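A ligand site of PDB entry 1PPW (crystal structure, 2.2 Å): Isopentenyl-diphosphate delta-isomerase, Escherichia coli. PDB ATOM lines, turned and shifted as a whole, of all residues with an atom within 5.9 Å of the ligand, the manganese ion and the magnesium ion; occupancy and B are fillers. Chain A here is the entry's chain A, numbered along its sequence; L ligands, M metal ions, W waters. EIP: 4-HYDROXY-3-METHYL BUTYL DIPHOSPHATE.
Water W1 lies within hydrogen-bond range of OE1 of Glu 87 (2.8 Å) and N of Cys 67 (2.9 Å).
Water W3 lies within hydrogen-bond range of O2 of the ligand (2.6 Å), N of His 69 (2.9 Å), OE2 of Glu 4 (3.0 Å) and NE of Arg 83 (3.2 Å).
The manganese ion is bound by NE2 of His 69 (2.0 Å), NE2 of His 32 (2.0 Å), NE2 of His 25 (2.1 Å), OE2 of Glu 116 (2.1 Å), OE1 of Glu 114 (2.2 Å) and OE2 of Glu 114 (2.3 Å).
The manganese ion has six donor atoms within binding distance.
Of the 28 residues printed, 2 come within 4 Å of the magnesium ion.
The nearest printed residue that does not touch the magnesium ion is Arg 83 (4.3 Å).
The backbone NH (N) of His 32 is in hydrogen-bond range of the backbone carbonyl oxygen (O) of Asn 115, 3.0 Å away.
A ring nitrogen (ND1) of His 25 sits at hydrogen-bond distance from the backbone carbonyl oxygen (O) of Lys 21 (3.1 Å).
The side-chain sulfur of Cys 67 is in hydrogen-bond range of the indole nitrogen of Trp 161, at 3.5 Å.
SG of Cys 67 sits at hydrogen-bond distance from OD1 of Asn 64 (3.5 Å).
SG of Cys 118 sits at hydrogen-bond distance from OG of Ser 36, 3.4 Å away.
NH2 of Arg 51 lies within hydrogen-bond range of O of Ala 57, at 2.7 Å.
The side-chain carboxylate of Glu 4 is in salt-bridge range of the side-chain amino group of Lys 21 (2.9 Å).
The side-chain carboxylate (OE1) of Glu 4 lies within salt-bridge range of the guanidinium group (NH1) of Arg 83 (3.8 Å).
Of the 28 residues printed, 5 come within 4 Å of the manganese ion.
The nearest printed residue that does not touch the manganese ion is Val 6 (5.0 Å).
An oxygen (O5) of the ligand lies within hydrogen-bond range of a ring nitrogen (ND1) of His 69 (3.2 Å).
The side-chain sulfur (SG) of Cys 67 sits at hydrogen-bond distance from an oxygen (O15) of the ligand (3.4 Å).
The side-chain hydroxyl of Ser 36 is in hydrogen-bond range of an oxygen (O15) of the ligand (2.5 Å).
An oxygen (O1) of the ligand is in salt-bridge range of the side-chain amino group of Lys 55 (2.7 Å).
The guanidinium group of Arg 51 is in salt-bridge range of an oxygen (O6) of the ligand, at 3.0 Å.
An oxygen (O15) of the ligand lies close to the indole nitrogen (NE1) of Trp 161 (3.1 Å).
An oxygen (O2) of the ligand is in salt-bridge range of the side-chain amino group of Lys 21.
The guanidinium group (NH2) of Arg 83 lies within salt-bridge range of an oxygen (O2) of the ligand (3.9 Å).
SG of Cys 118 sits at hydrogen-bond distance from O15 of the ligand (3.7 Å).
Ala 34 touches the ligand.
O of Phe 35 touches C14 of the ligand (3.5 Å).
Gly 68 touches the ligand.
OH of Tyr 104 touches C13 of the ligand (2.8 Å).
Of the 28 residues printed, 16 come within 4 Å of the ligand.
O3 of the ligand is bound to the magnesium ion, 2.0 Å away.
The magnesium ion is bound by water W1, 2.1 Å away.
The magnesium ion is bound by O7 of the ligand, 2.1 Å away.
OE2 of Glu 87 binds the magnesium ion.
The magnesium ion is bound by O of Cys 67 (2.3 Å).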
ATOM      1  N   GLU A   4      15.300  17.350 -30.606  1.00  0.00           N
ATOM      2  CA  GLU A   4      15.769  16.459 -29.562  1.00  0.00           C
ATOM      3  C   GLU A   4      16.147  17.233 -28.299  1.00  0.00           C
ATOM      4  O   GLU A   4      16.427  18.433 -28.298  1.00  0.00           O
ATOM      5  CB  GLU A   4      16.956  15.612 -30.066  1.00  0.00           C
ATOM      6  CG  GLU A   4      17.288  14.456 -29.128  1.00  0.00           C
ATOM      7  CD  GLU A   4      18.402  13.558 -29.642  1.00  0.00           C
ATOM      8  OE1 GLU A   4      18.972  13.894 -30.700  1.00  0.00           O
ATOM      9  OE2 GLU A   4      18.683  12.528 -28.973  1.00  0.00           O
ATOM     10  N   VAL A   6      17.645  16.686 -23.865  1.00  0.00           N
ATOM     11  CA  VAL A   6      18.244  15.902 -22.789  1.00  0.00           C
ATOM     12  C   VAL A   6      17.357  15.984 -21.559  1.00  0.00           C
ATOM     13  O   VAL A   6      16.566  16.927 -21.410  1.00  0.00           O
ATOM     14  CB  VAL A   6      19.669  16.384 -22.476  1.00  0.00           C
ATOM     15  CG1 VAL A   6      20.448  16.552 -23.780  1.00  0.00           C
ATOM     16  CG2 VAL A   6      19.681  17.684 -21.687  1.00  0.00           C
ATOM     17  N   LYS A  21      18.992  19.748 -27.041  1.00  0.00           N
ATOM     18  CA  LYS A  21      20.261  19.039 -26.863  1.00  0.00           C
ATOM     19  C   LYS A  21      21.472  19.919 -27.135  1.00  0.00           C
ATOM     20  O   LYS A  21      22.419  19.912 -26.347  1.00  0.00           O
ATOM     21  CB  LYS A  21      20.299  17.801 -27.766  1.00  0.00           C
ATOM     22  CG  LYS A  21      21.499  16.899 -27.571  1.00  0.00           C
ATOM     23  CD  LYS A  21      21.410  15.630 -28.398  1.00  0.00           C
ATOM     24  CE  LYS A  21      21.987  15.826 -29.798  1.00  0.00           C
ATOM     25  NZ  LYS A  21      21.820  14.608 -30.641  1.00  0.00           N
ATOM     26  N   HIS A  25      24.759  21.368 -23.861  1.00  0.00           N
ATOM     27  CA  HIS A  25      26.174  21.061 -23.575  1.00  0.00           C
ATOM     28  C   HIS A  25      27.015  22.323 -23.652  1.00  0.00           C
ATOM     29  O   HIS A  25      27.244  22.921 -24.713  1.00  0.00           O
ATOM     30  CB  HIS A  25      26.612  19.947 -24.525  1.00  0.00           C
ATOM     31  CG  HIS A  25      25.855  18.669 -24.267  1.00  0.00           C
ATOM     32  ND1 HIS A  25      24.718  18.307 -24.948  1.00  0.00           N
ATOM     33  CD2 HIS A  25      26.074  17.679 -23.369  1.00  0.00           C
ATOM     34  CE1 HIS A  25      24.274  17.145 -24.492  1.00  0.00           C
ATOM     35  NE2 HIS A  25      25.089  16.736 -23.519  1.00  0.00           N
ATOM     36  N   THR A  29      27.651  22.470 -18.176  1.00  0.00           N
ATOM     37  CA  THR A  29      26.557  21.519 -18.382  1.00  0.00           C
ATOM     38  C   THR A  29      25.968  20.997 -17.080  1.00  0.00           C
ATOM     39  O   THR A  29      26.684  20.602 -16.162  1.00  0.00           O
ATOM     40  CB  THR A  29      27.019  20.321 -19.231  1.00  0.00           C
ATOM     41  OG1 THR A  29      27.447  20.801 -20.504  1.00  0.00           O
ATOM     42  CG2 THR A  29      25.864  19.363 -19.453  1.00  0.00           C
ATOM     43  N   HIS A  32      22.434  15.443 -16.485  1.00  0.00           N
ATOM     44  CA  HIS A  32      21.317  14.950 -17.279  1.00  0.00           C
ATOM     45  C   HIS A  32      21.461  13.452 -17.560  1.00  0.00           C
ATOM     46  O   HIS A  32      22.475  12.856 -17.177  1.00  0.00           O
ATOM     47  CB  HIS A  32      21.214  15.725 -18.586  1.00  0.00           C
ATOM     48  CG  HIS A  32      22.382  15.796 -19.501  1.00  0.00           C
ATOM     49  ND1 HIS A  32      23.380  16.741 -19.399  1.00  0.00           N
ATOM     50  CD2 HIS A  32      22.712  15.045 -20.589  1.00  0.00           C
ATOM     51  CE1 HIS A  32      24.278  16.564 -20.351  1.00  0.00           C
ATOM     52  NE2 HIS A  32      23.898  15.541 -21.090  1.00  0.00           N
ATOM     53  N   LEU A  33      20.458  12.868 -18.192  1.00  0.00           N
ATOM     54  CA  LEU A  33      20.403  11.462 -18.545  1.00  0.00           C
ATOM     55  C   LEU A  33      21.129  11.130 -19.842  1.00  0.00           C
ATOM     56  O   LEU A  33      21.018  11.879 -20.807  1.00  0.00           O
ATOM     57  CB  LEU A  33      18.928  11.042 -18.707  1.00  0.00           C
ATOM     58  CG  LEU A  33      18.601   9.578 -18.375  1.00  0.00           C
ATOM     59  CD1 LEU A  33      19.096   9.206 -16.993  1.00  0.00           C
ATOM     60  CD2 LEU A  33      17.105   9.360 -18.501  1.00  0.00           C
ATOM     61  N   ALA A  34      21.821   9.998 -19.863  1.00  0.00           N
ATOM     62  CA  ALA A  34      22.474   9.505 -21.071  1.00  0.00           C
ATOM     63  C   ALA A  34      22.690   7.990 -21.072  1.00  0.00           C
ATOM     64  O   ALA A  34      22.435   7.343 -20.057  1.00  0.00           O
ATOM     65  CB  ALA A  34      23.827  10.186 -21.242  1.00  0.00           C
ATOM     66  N   PHE A  35      23.167   7.452 -22.188  1.00  0.00           N
ATOM     67  CA  PHE A  35      23.598   6.065 -22.238  1.00  0.00           C
ATOM     68  C   PHE A  35      24.954   5.930 -22.933  1.00  0.00           C
ATOM     69  O   PHE A  35      25.300   6.759 -23.777  1.00  0.00           O
ATOM     70  CB  PHE A  35      22.623   5.145 -22.971  1.00  0.00           C
ATOM     71  CG  PHE A  35      22.493   5.392 -24.474  1.00  0.00           C
ATOM     72  CD1 PHE A  35      23.237   4.720 -25.444  1.00  0.00           C
ATOM     73  CD2 PHE A  35      21.566   6.341 -24.883  1.00  0.00           C
ATOM     74  CE1 PHE A  35      23.096   4.988 -26.791  1.00  0.00           C
ATOM     75  CE2 PHE A  35      21.398   6.602 -26.233  1.00  0.00           C
ATOM     76  CZ  PHE A  35      22.149   5.922 -27.182  1.00  0.00           C
ATOM     77  N   SER A  36      25.644   4.845 -22.633  1.00  0.00           N
ATOM     78  CA  SER A  36      26.798   4.428 -23.421  1.00  0.00           C
ATOM     79  C   SER A  36      26.522   3.023 -23.952  1.00  0.00           C
ATOM     80  O   SER A  36      25.769   2.259 -23.351  1.00  0.00           O
ATOM     81  CB  SER A  36      28.097   4.452 -22.625  1.00  0.00           C
ATOM     82  OG  SER A  36      28.695   5.745 -22.653  1.00  0.00           O
ATOM     83  N   ARG A  51      34.426  10.238 -33.009  1.00  0.00           N
ATOM     84  CA  ARG A  51      33.359  11.228 -33.157  1.00  0.00           C
ATOM     85  C   ARG A  51      33.701  12.248 -34.241  1.00  0.00           C
ATOM     86  O   ARG A  51      34.849  12.691 -34.334  1.00  0.00           O
ATOM     87  CB  ARG A  51      33.092  11.887 -31.806  1.00  0.00           C
ATOM     88  CG  ARG A  51      32.715  10.952 -30.676  1.00  0.00           C
ATOM     89  CD  ARG A  51      32.929  11.634 -29.322  1.00  0.00           C
ATOM     90  NE  ARG A  51      32.059  12.786 -29.108  1.00  0.00           N
ATOM     91  CZ  ARG A  51      30.746  12.715 -28.895  1.00  0.00           C
ATOM     92  NH1 ARG A  51      30.109  11.546 -28.877  1.00  0.00           N
ATOM     93  NH2 ARG A  51      30.020  13.811 -28.701  1.00  0.00           N
ATOM     94  N   LYS A  55      30.906  17.295 -33.753  1.00  0.00           N
ATOM     95  CA  LYS A  55      30.208  17.086 -32.474  1.00  0.00           C
ATOM     96  C   LYS A  55      30.485  18.211 -31.491  1.00  0.00           C
ATOM     97  O   LYS A  55      31.550  18.820 -31.457  1.00  0.00           O
ATOM     98  CB  LYS A  55      30.595  15.741 -31.867  1.00  0.00           C
ATOM     99  CG  LYS A  55      30.277  14.585 -32.813  1.00  0.00           C
ATOM    100  CD  LYS A  55      29.048  13.807 -32.371  1.00  0.00           C
ATOM    101  CE  LYS A  55      27.814  14.684 -32.371  1.00  0.00           C
ATOM    102  NZ  LYS A  55      26.662  14.066 -31.654  1.00  0.00           N
ATOM    103  N   ALA A  57      30.582  18.094 -28.102  1.00  0.00           N
ATOM    104  CA  ALA A  57      31.485  17.605 -27.077  1.00  0.00           C
ATOM    105  C   ALA A  57      32.399  16.510 -27.640  1.00  0.00           C
ATOM    106  O   ALA A  57      31.938  15.662 -28.393  1.00  0.00           O
ATOM    107  CB  ALA A  57      30.706  17.073 -25.884  1.00  0.00           C
ATOM    108  N   ASN A  64      33.848   4.501 -27.286  1.00  0.00           N
ATOM    109  CA  ASN A  64      33.139   3.246 -27.563  1.00  0.00           C
ATOM    110  C   ASN A  64      32.111   3.462 -28.664  1.00  0.00           C
ATOM    111  O   ASN A  64      32.000   4.549 -29.234  1.00  0.00           O
ATOM    112  CB  ASN A  64      32.501   2.700 -26.295  1.00  0.00           C
ATOM    113  CG  ASN A  64      31.629   3.766 -25.656  1.00  0.00           C
ATOM    114  OD1 ASN A  64      30.410   3.756 -25.780  1.00  0.00           O
ATOM    115  ND2 ASN A  64      32.300   4.699 -24.990  1.00  0.00           N
ATOM    116  N   VAL A  66      28.632   3.592 -29.496  1.00  0.00           N
ATOM    117  CA  VAL A  66      27.542   4.565 -29.662  1.00  0.00           C
ATOM    118  C   VAL A  66      27.176   5.116 -28.289  1.00  0.00           C
ATOM    119  O   VAL A  66      27.149   4.352 -27.320  1.00  0.00           O
ATOM    120  CB  VAL A  66      26.363   3.881 -30.382  1.00  0.00           C
ATOM    121  CG1 VAL A  66      25.932   2.647 -29.604  1.00  0.00           C
ATOM    122  CG2 VAL A  66      25.199   4.835 -30.564  1.00  0.00           C
ATOM    123  N   CYS A  67      26.925   6.416 -28.203  1.00  0.00           N
ATOM    124  CA  CYS A  67      26.572   7.133 -26.991  1.00  0.00           C
ATOM    125  C   CYS A  67      25.389   8.049 -27.290  1.00  0.00           C
ATOM    126  O   CYS A  67      25.261   8.479 -28.440  1.00  0.00           O
ATOM    127  CB  CYS A  67      27.756   7.929 -26.426  1.00  0.00           C
ATOM    128  SG  CYS A  67      29.319   7.007 -26.257  1.00  0.00           S
ATOM    129  N   GLY A  68      24.531   8.349 -26.331  1.00  0.00           N
ATOM    130  CA  GLY A  68      23.391   9.204 -26.612  1.00  0.00           C
ATOM    131  C   GLY A  68      22.572   9.633 -25.419  1.00  0.00           C
ATOM    132  O   GLY A  68      22.936   9.471 -24.249  1.00  0.00           O
ATOM    133  N   HIS A  69      21.414  10.224 -25.705  1.00  0.00           N
ATOM    134  CA  HIS A  69      20.560  10.857 -24.720  1.00  0.00           C
ATOM    135  C   HIS A  69      19.105  10.402 -24.851  1.00  0.00           C
ATOM    136  O   HIS A  69      18.387  10.807 -25.769  1.00  0.00           O
ATOM    137  CB  HIS A  69      20.644  12.385 -24.895  1.00  0.00           C
ATOM    138  CG  HIS A  69      21.979  12.978 -24.578  1.00  0.00           C
ATOM    139  ND1 HIS A  69      22.890  13.331 -25.564  1.00  0.00           N
ATOM    140  CD2 HIS A  69      22.564  13.288 -23.396  1.00  0.00           C
ATOM    141  CE1 HIS A  69      23.967  13.830 -24.995  1.00  0.00           C
ATOM    142  NE2 HIS A  69      23.800  13.822 -23.676  1.00  0.00           N
ATOM    143  N   ARG A  83      19.834   5.327 -31.520  1.00  0.00           N
ATOM    144  CA  ARG A  83      21.058   5.990 -31.971  1.00  0.00           C
ATOM    145  C   ARG A  83      21.917   5.040 -32.803  1.00  0.00           C
ATOM    146  O   ARG A  83      22.717   5.482 -33.624  1.00  0.00           O
ATOM    147  CB  ARG A  83      21.809   6.550 -30.765  1.00  0.00           C
ATOM    148  CG  ARG A  83      21.071   7.663 -30.058  1.00  0.00           C
ATOM    149  CD  ARG A  83      20.723   8.784 -31.027  1.00  0.00           C
ATOM    150  NE  ARG A  83      21.900   9.570 -31.418  1.00  0.00           N
ATOM    151  CZ  ARG A  83      21.821  10.640 -32.198  1.00  0.00           C
ATOM    152  NH1 ARG A  83      20.633  11.034 -32.647  1.00  0.00           N
ATOM    153  NH2 ARG A  83      22.901  11.319 -32.531  1.00  0.00           N
ATOM    154  N   GLU A  87      23.236   6.784 -35.864  1.00  0.00           N
ATOM    155  CA  GLU A  87      24.625   7.172 -36.177  1.00  0.00           C
ATOM    156  C   GLU A  87      25.309   6.165 -37.082  1.00  0.00           C
ATOM    157  O   GLU A  87      26.176   6.553 -37.852  1.00  0.00           O
ATOM    158  CB  GLU A  87      25.430   7.376 -34.884  1.00  0.00           C
ATOM    159  CG  GLU A  87      24.619   8.156 -33.849  1.00  0.00           C
ATOM    160  CD  GLU A  87      25.412   8.356 -32.571  1.00  0.00           C
ATOM    161  OE1 GLU A  87      26.533   7.802 -32.531  1.00  0.00           O
ATOM    162  OE2 GLU A  87      24.897   9.025 -31.657  1.00  0.00           O
ATOM    163  N   TYR A 104      29.203  10.397 -14.474  1.00  0.00           N
ATOM    164  CA  TYR A 104      30.447  11.122 -14.637  1.00  0.00           C
ATOM    165  C   TYR A 104      30.210  12.560 -15.110  1.00  0.00           C
ATOM    166  O   TYR A 104      29.247  12.864 -15.811  1.00  0.00           O
ATOM    167  CB  TYR A 104      31.367  10.423 -15.657  1.00  0.00           C
ATOM    168  CG  TYR A 104      31.029  10.783 -17.092  1.00  0.00           C
ATOM    169  CD1 TYR A 104      31.825  11.648 -17.836  1.00  0.00           C
ATOM    170  CD2 TYR A 104      29.899  10.258 -17.717  1.00  0.00           C
ATOM    171  CE1 TYR A 104      31.512  11.986 -19.132  1.00  0.00           C
ATOM    172  CE2 TYR A 104      29.575  10.583 -19.015  1.00  0.00           C
ATOM    173  CZ  TYR A 104      30.387  11.453 -19.721  1.00  0.00           C
ATOM    174  OH  TYR A 104      30.095  11.797 -21.022  1.00  0.00           O
ATOM    175  N   GLU A 114      30.598  17.289 -20.158  1.00  0.00           N
ATOM    176  CA  GLU A 114      29.517  16.316 -20.064  1.00  0.00           C
ATOM    177  C   GLU A 114      29.359  16.014 -18.562  1.00  0.00           C
ATOM    178  O   GLU A 114      30.360  15.824 -17.877  1.00  0.00           O
ATOM    179  CB  GLU A 114      29.705  15.017 -20.813  1.00  0.00           C
ATOM    180  CG  GLU A 114      29.127  14.953 -22.205  1.00  0.00           C
ATOM    181  CD  GLU A 114      27.608  14.937 -22.281  1.00  0.00           C
ATOM    182  OE1 GLU A 114      27.106  14.650 -23.402  1.00  0.00           O
ATOM    183  OE2 GLU A 114      26.926  15.500 -21.396  1.00  0.00           O
ATOM    184  N   ASN A 115      28.106  15.984 -18.149  1.00  0.00           N
ATOM    185  CA  ASN A 115      27.711  15.742 -16.762  1.00  0.00           C
ATOM    186  C   ASN A 115      26.495  14.824 -16.770  1.00  0.00           C
ATOM    187  O   ASN A 115      25.351  15.256 -16.957  1.00  0.00           O
ATOM    188  CB  ASN A 115      27.437  17.078 -16.109  1.00  0.00           C
ATOM    189  CG  ASN A 115      27.208  17.047 -14.612  1.00  0.00           C
ATOM    190  OD1 ASN A 115      27.376  16.018 -13.971  1.00  0.00           O
ATOM    191  ND2 ASN A 115      26.841  18.202 -14.065  1.00  0.00           N
ATOM    192  N   GLU A 116      26.736  13.526 -16.607  1.00  0.00           N
ATOM    193  CA  GLU A 116      25.686  12.574 -16.922  1.00  0.00           C
ATOM    194  C   GLU A 116      25.543  11.417 -15.958  1.00  0.00           C
ATOM    195  O   GLU A 116      26.508  10.895 -15.403  1.00  0.00           O
ATOM    196  CB  GLU A 116      25.944  11.973 -18.331  1.00  0.00           C
ATOM    197  CG  GLU A 116      25.804  13.011 -19.425  1.00  0.00           C
ATOM    198  CD  GLU A 116      26.116  12.508 -20.818  1.00  0.00           C
ATOM    199  OE1 GLU A 116      26.913  11.556 -20.945  1.00  0.00           O
ATOM    200  OE2 GLU A 116      25.550  13.076 -21.772  1.00  0.00           O
ATOM    201  N   CYS A 118      24.840   7.932 -16.699  1.00  0.00           N
ATOM    202  CA  CYS A 118      25.027   7.305 -18.009  1.00  0.00           C
ATOM    203  C   CYS A 118      25.163   5.792 -17.913  1.00  0.00           C
ATOM    204  O   CYS A 118      26.296   5.322 -17.963  1.00  0.00           O
ATOM    205  CB  CYS A 118      26.269   7.927 -18.630  1.00  0.00           C
ATOM    206  SG  CYS A 118      26.765   7.241 -20.223  1.00  0.00           S
ATOM    207  N   GLU A 135      27.965  12.091 -37.568  1.00  0.00           N
ATOM    208  CA  GLU A 135      28.207  11.601 -36.212  1.00  0.00           C
ATOM    209  C   GLU A 135      29.541  10.888 -36.069  1.00  0.00           C
ATOM    210  O   GLU A 135      30.241  11.018 -35.075  1.00  0.00           O
ATOM    211  CB  GLU A 135      27.073  10.662 -35.782  1.00  0.00           C
ATOM    212  CG  GLU A 135      25.679  11.256 -35.955  1.00  0.00           C
ATOM    213  CD  GLU A 135      25.415  12.283 -34.862  1.00  0.00           C
ATOM    214  OE1 GLU A 135      26.048  12.159 -33.802  1.00  0.00           O
ATOM    215  OE2 GLU A 135      24.602  13.204 -35.073  1.00  0.00           O
ATOM    216  N   TRP A 161      34.950   8.957 -20.689  1.00  0.00           N
ATOM    217  CA  TRP A 161      33.951   8.014 -20.156  1.00  0.00           C
ATOM    218  C   TRP A 161      34.254   6.605 -20.650  1.00  0.00           C
ATOM    219  O   TRP A 161      34.003   5.602 -19.968  1.00  0.00           O
ATOM    220  CB  TRP A 161      32.521   8.440 -20.507  1.00  0.00           C
ATOM    221  CG  TRP A 161      32.315   8.647 -21.970  1.00  0.00           C
ATOM    222  CD1 TRP A 161      31.785   7.768 -22.867  1.00  0.00           C
ATOM    223  CD2 TRP A 161      32.658   9.829 -22.709  1.00  0.00           C
ATOM    224  NE1 TRP A 161      31.767   8.339 -24.130  1.00  0.00           N
ATOM    225  CE2 TRP A 161      32.303   9.597 -24.054  1.00  0.00           C
ATOM    226  CE3 TRP A 161      33.233  11.051 -22.350  1.00  0.00           C
ATOM    227  CZ2 TRP A 161      32.503  10.550 -25.042  1.00  0.00           C
ATOM    228  CZ3 TRP A 161      33.433  12.004 -23.338  1.00  0.00           C
ATOM    229  CH2 TRP A 161      33.059  11.747 -24.664  1.00  0.00           C
ATOM    230  N   GLN A 165      34.666   3.600 -18.031  1.00  0.00           N
ATOM    231  CA  GLN A 165      33.820   2.416 -18.081  1.00  0.00           C
ATOM    232  C   GLN A 165      34.649   1.153 -18.152  1.00  0.00           C
ATOM    233  O   GLN A 165      34.377   0.186 -17.436  1.00  0.00           O
ATOM    234  CB  GLN A 165      32.853   2.503 -19.277  1.00  0.00           C
ATOM    235  CG  GLN A 165      31.755   3.533 -19.044  1.00  0.00           C
ATOM    236  CD  GLN A 165      31.054   3.893 -20.346  1.00  0.00           C
ATOM    237  OE1 GLN A 165      31.001   3.087 -21.261  1.00  0.00           O
ATOM    238  NE2 GLN A 165      30.520   5.117 -20.424  1.00  0.00           N
HETATM  239  O1  EIP L   1      24.943  13.749 -29.614  1.00  0.00           O
HETATM  240  O2  EIP L   1      23.101  12.558 -28.891  1.00  0.00           O
HETATM  241  O3  EIP L   1      24.869  11.397 -29.940  1.00  0.00           O
HETATM  242  P4  EIP L   1      24.438  12.481 -28.988  1.00  0.00           P
HETATM  243  O5  EIP L   1      25.115  12.323 -27.623  1.00  0.00           O
HETATM  244  O6  EIP L   1      27.440  13.026 -27.487  1.00  0.00           O
HETATM  245  O7  EIP L   1      26.874  11.007 -28.568  1.00  0.00           O
HETATM  246  P8  EIP L   1      26.599  11.980 -27.457  1.00  0.00           P
HETATM  247  O9  EIP L   1      26.715  11.145 -26.185  1.00  0.00           O
HETATM  248  C10 EIP L   1      27.113  11.943 -25.070  1.00  0.00           C
HETATM  249  C11 EIP L   1      28.412  11.489 -24.386  1.00  0.00           C
HETATM  250  C12 EIP L   1      28.178  10.432 -23.489  1.00  0.00           C
HETATM  251  C13 EIP L   1      29.159   9.763 -22.698  1.00  0.00           C
HETATM  252  C14 EIP L   1      26.739   9.934 -23.369  1.00  0.00           C
HETATM  253  O15 EIP L   1      28.868   8.211 -23.098  1.00  0.00           O
HETATM  254 MN    MN M   1      25.046  14.892 -22.608  1.00  0.00          MN
HETATM  255 MG    MG M   2      26.102   9.835 -30.085  1.00  0.00          MG
HETATM  256  O   HOH W   1      27.675   8.511 -30.027  1.00  0.00           O
HETATM  257  O   HOH W   2      24.674  15.919 -28.129  1.00  0.00           O
HETATM  258  O   HOH W   3      21.183  10.864 -28.547  1.00  0.00           O
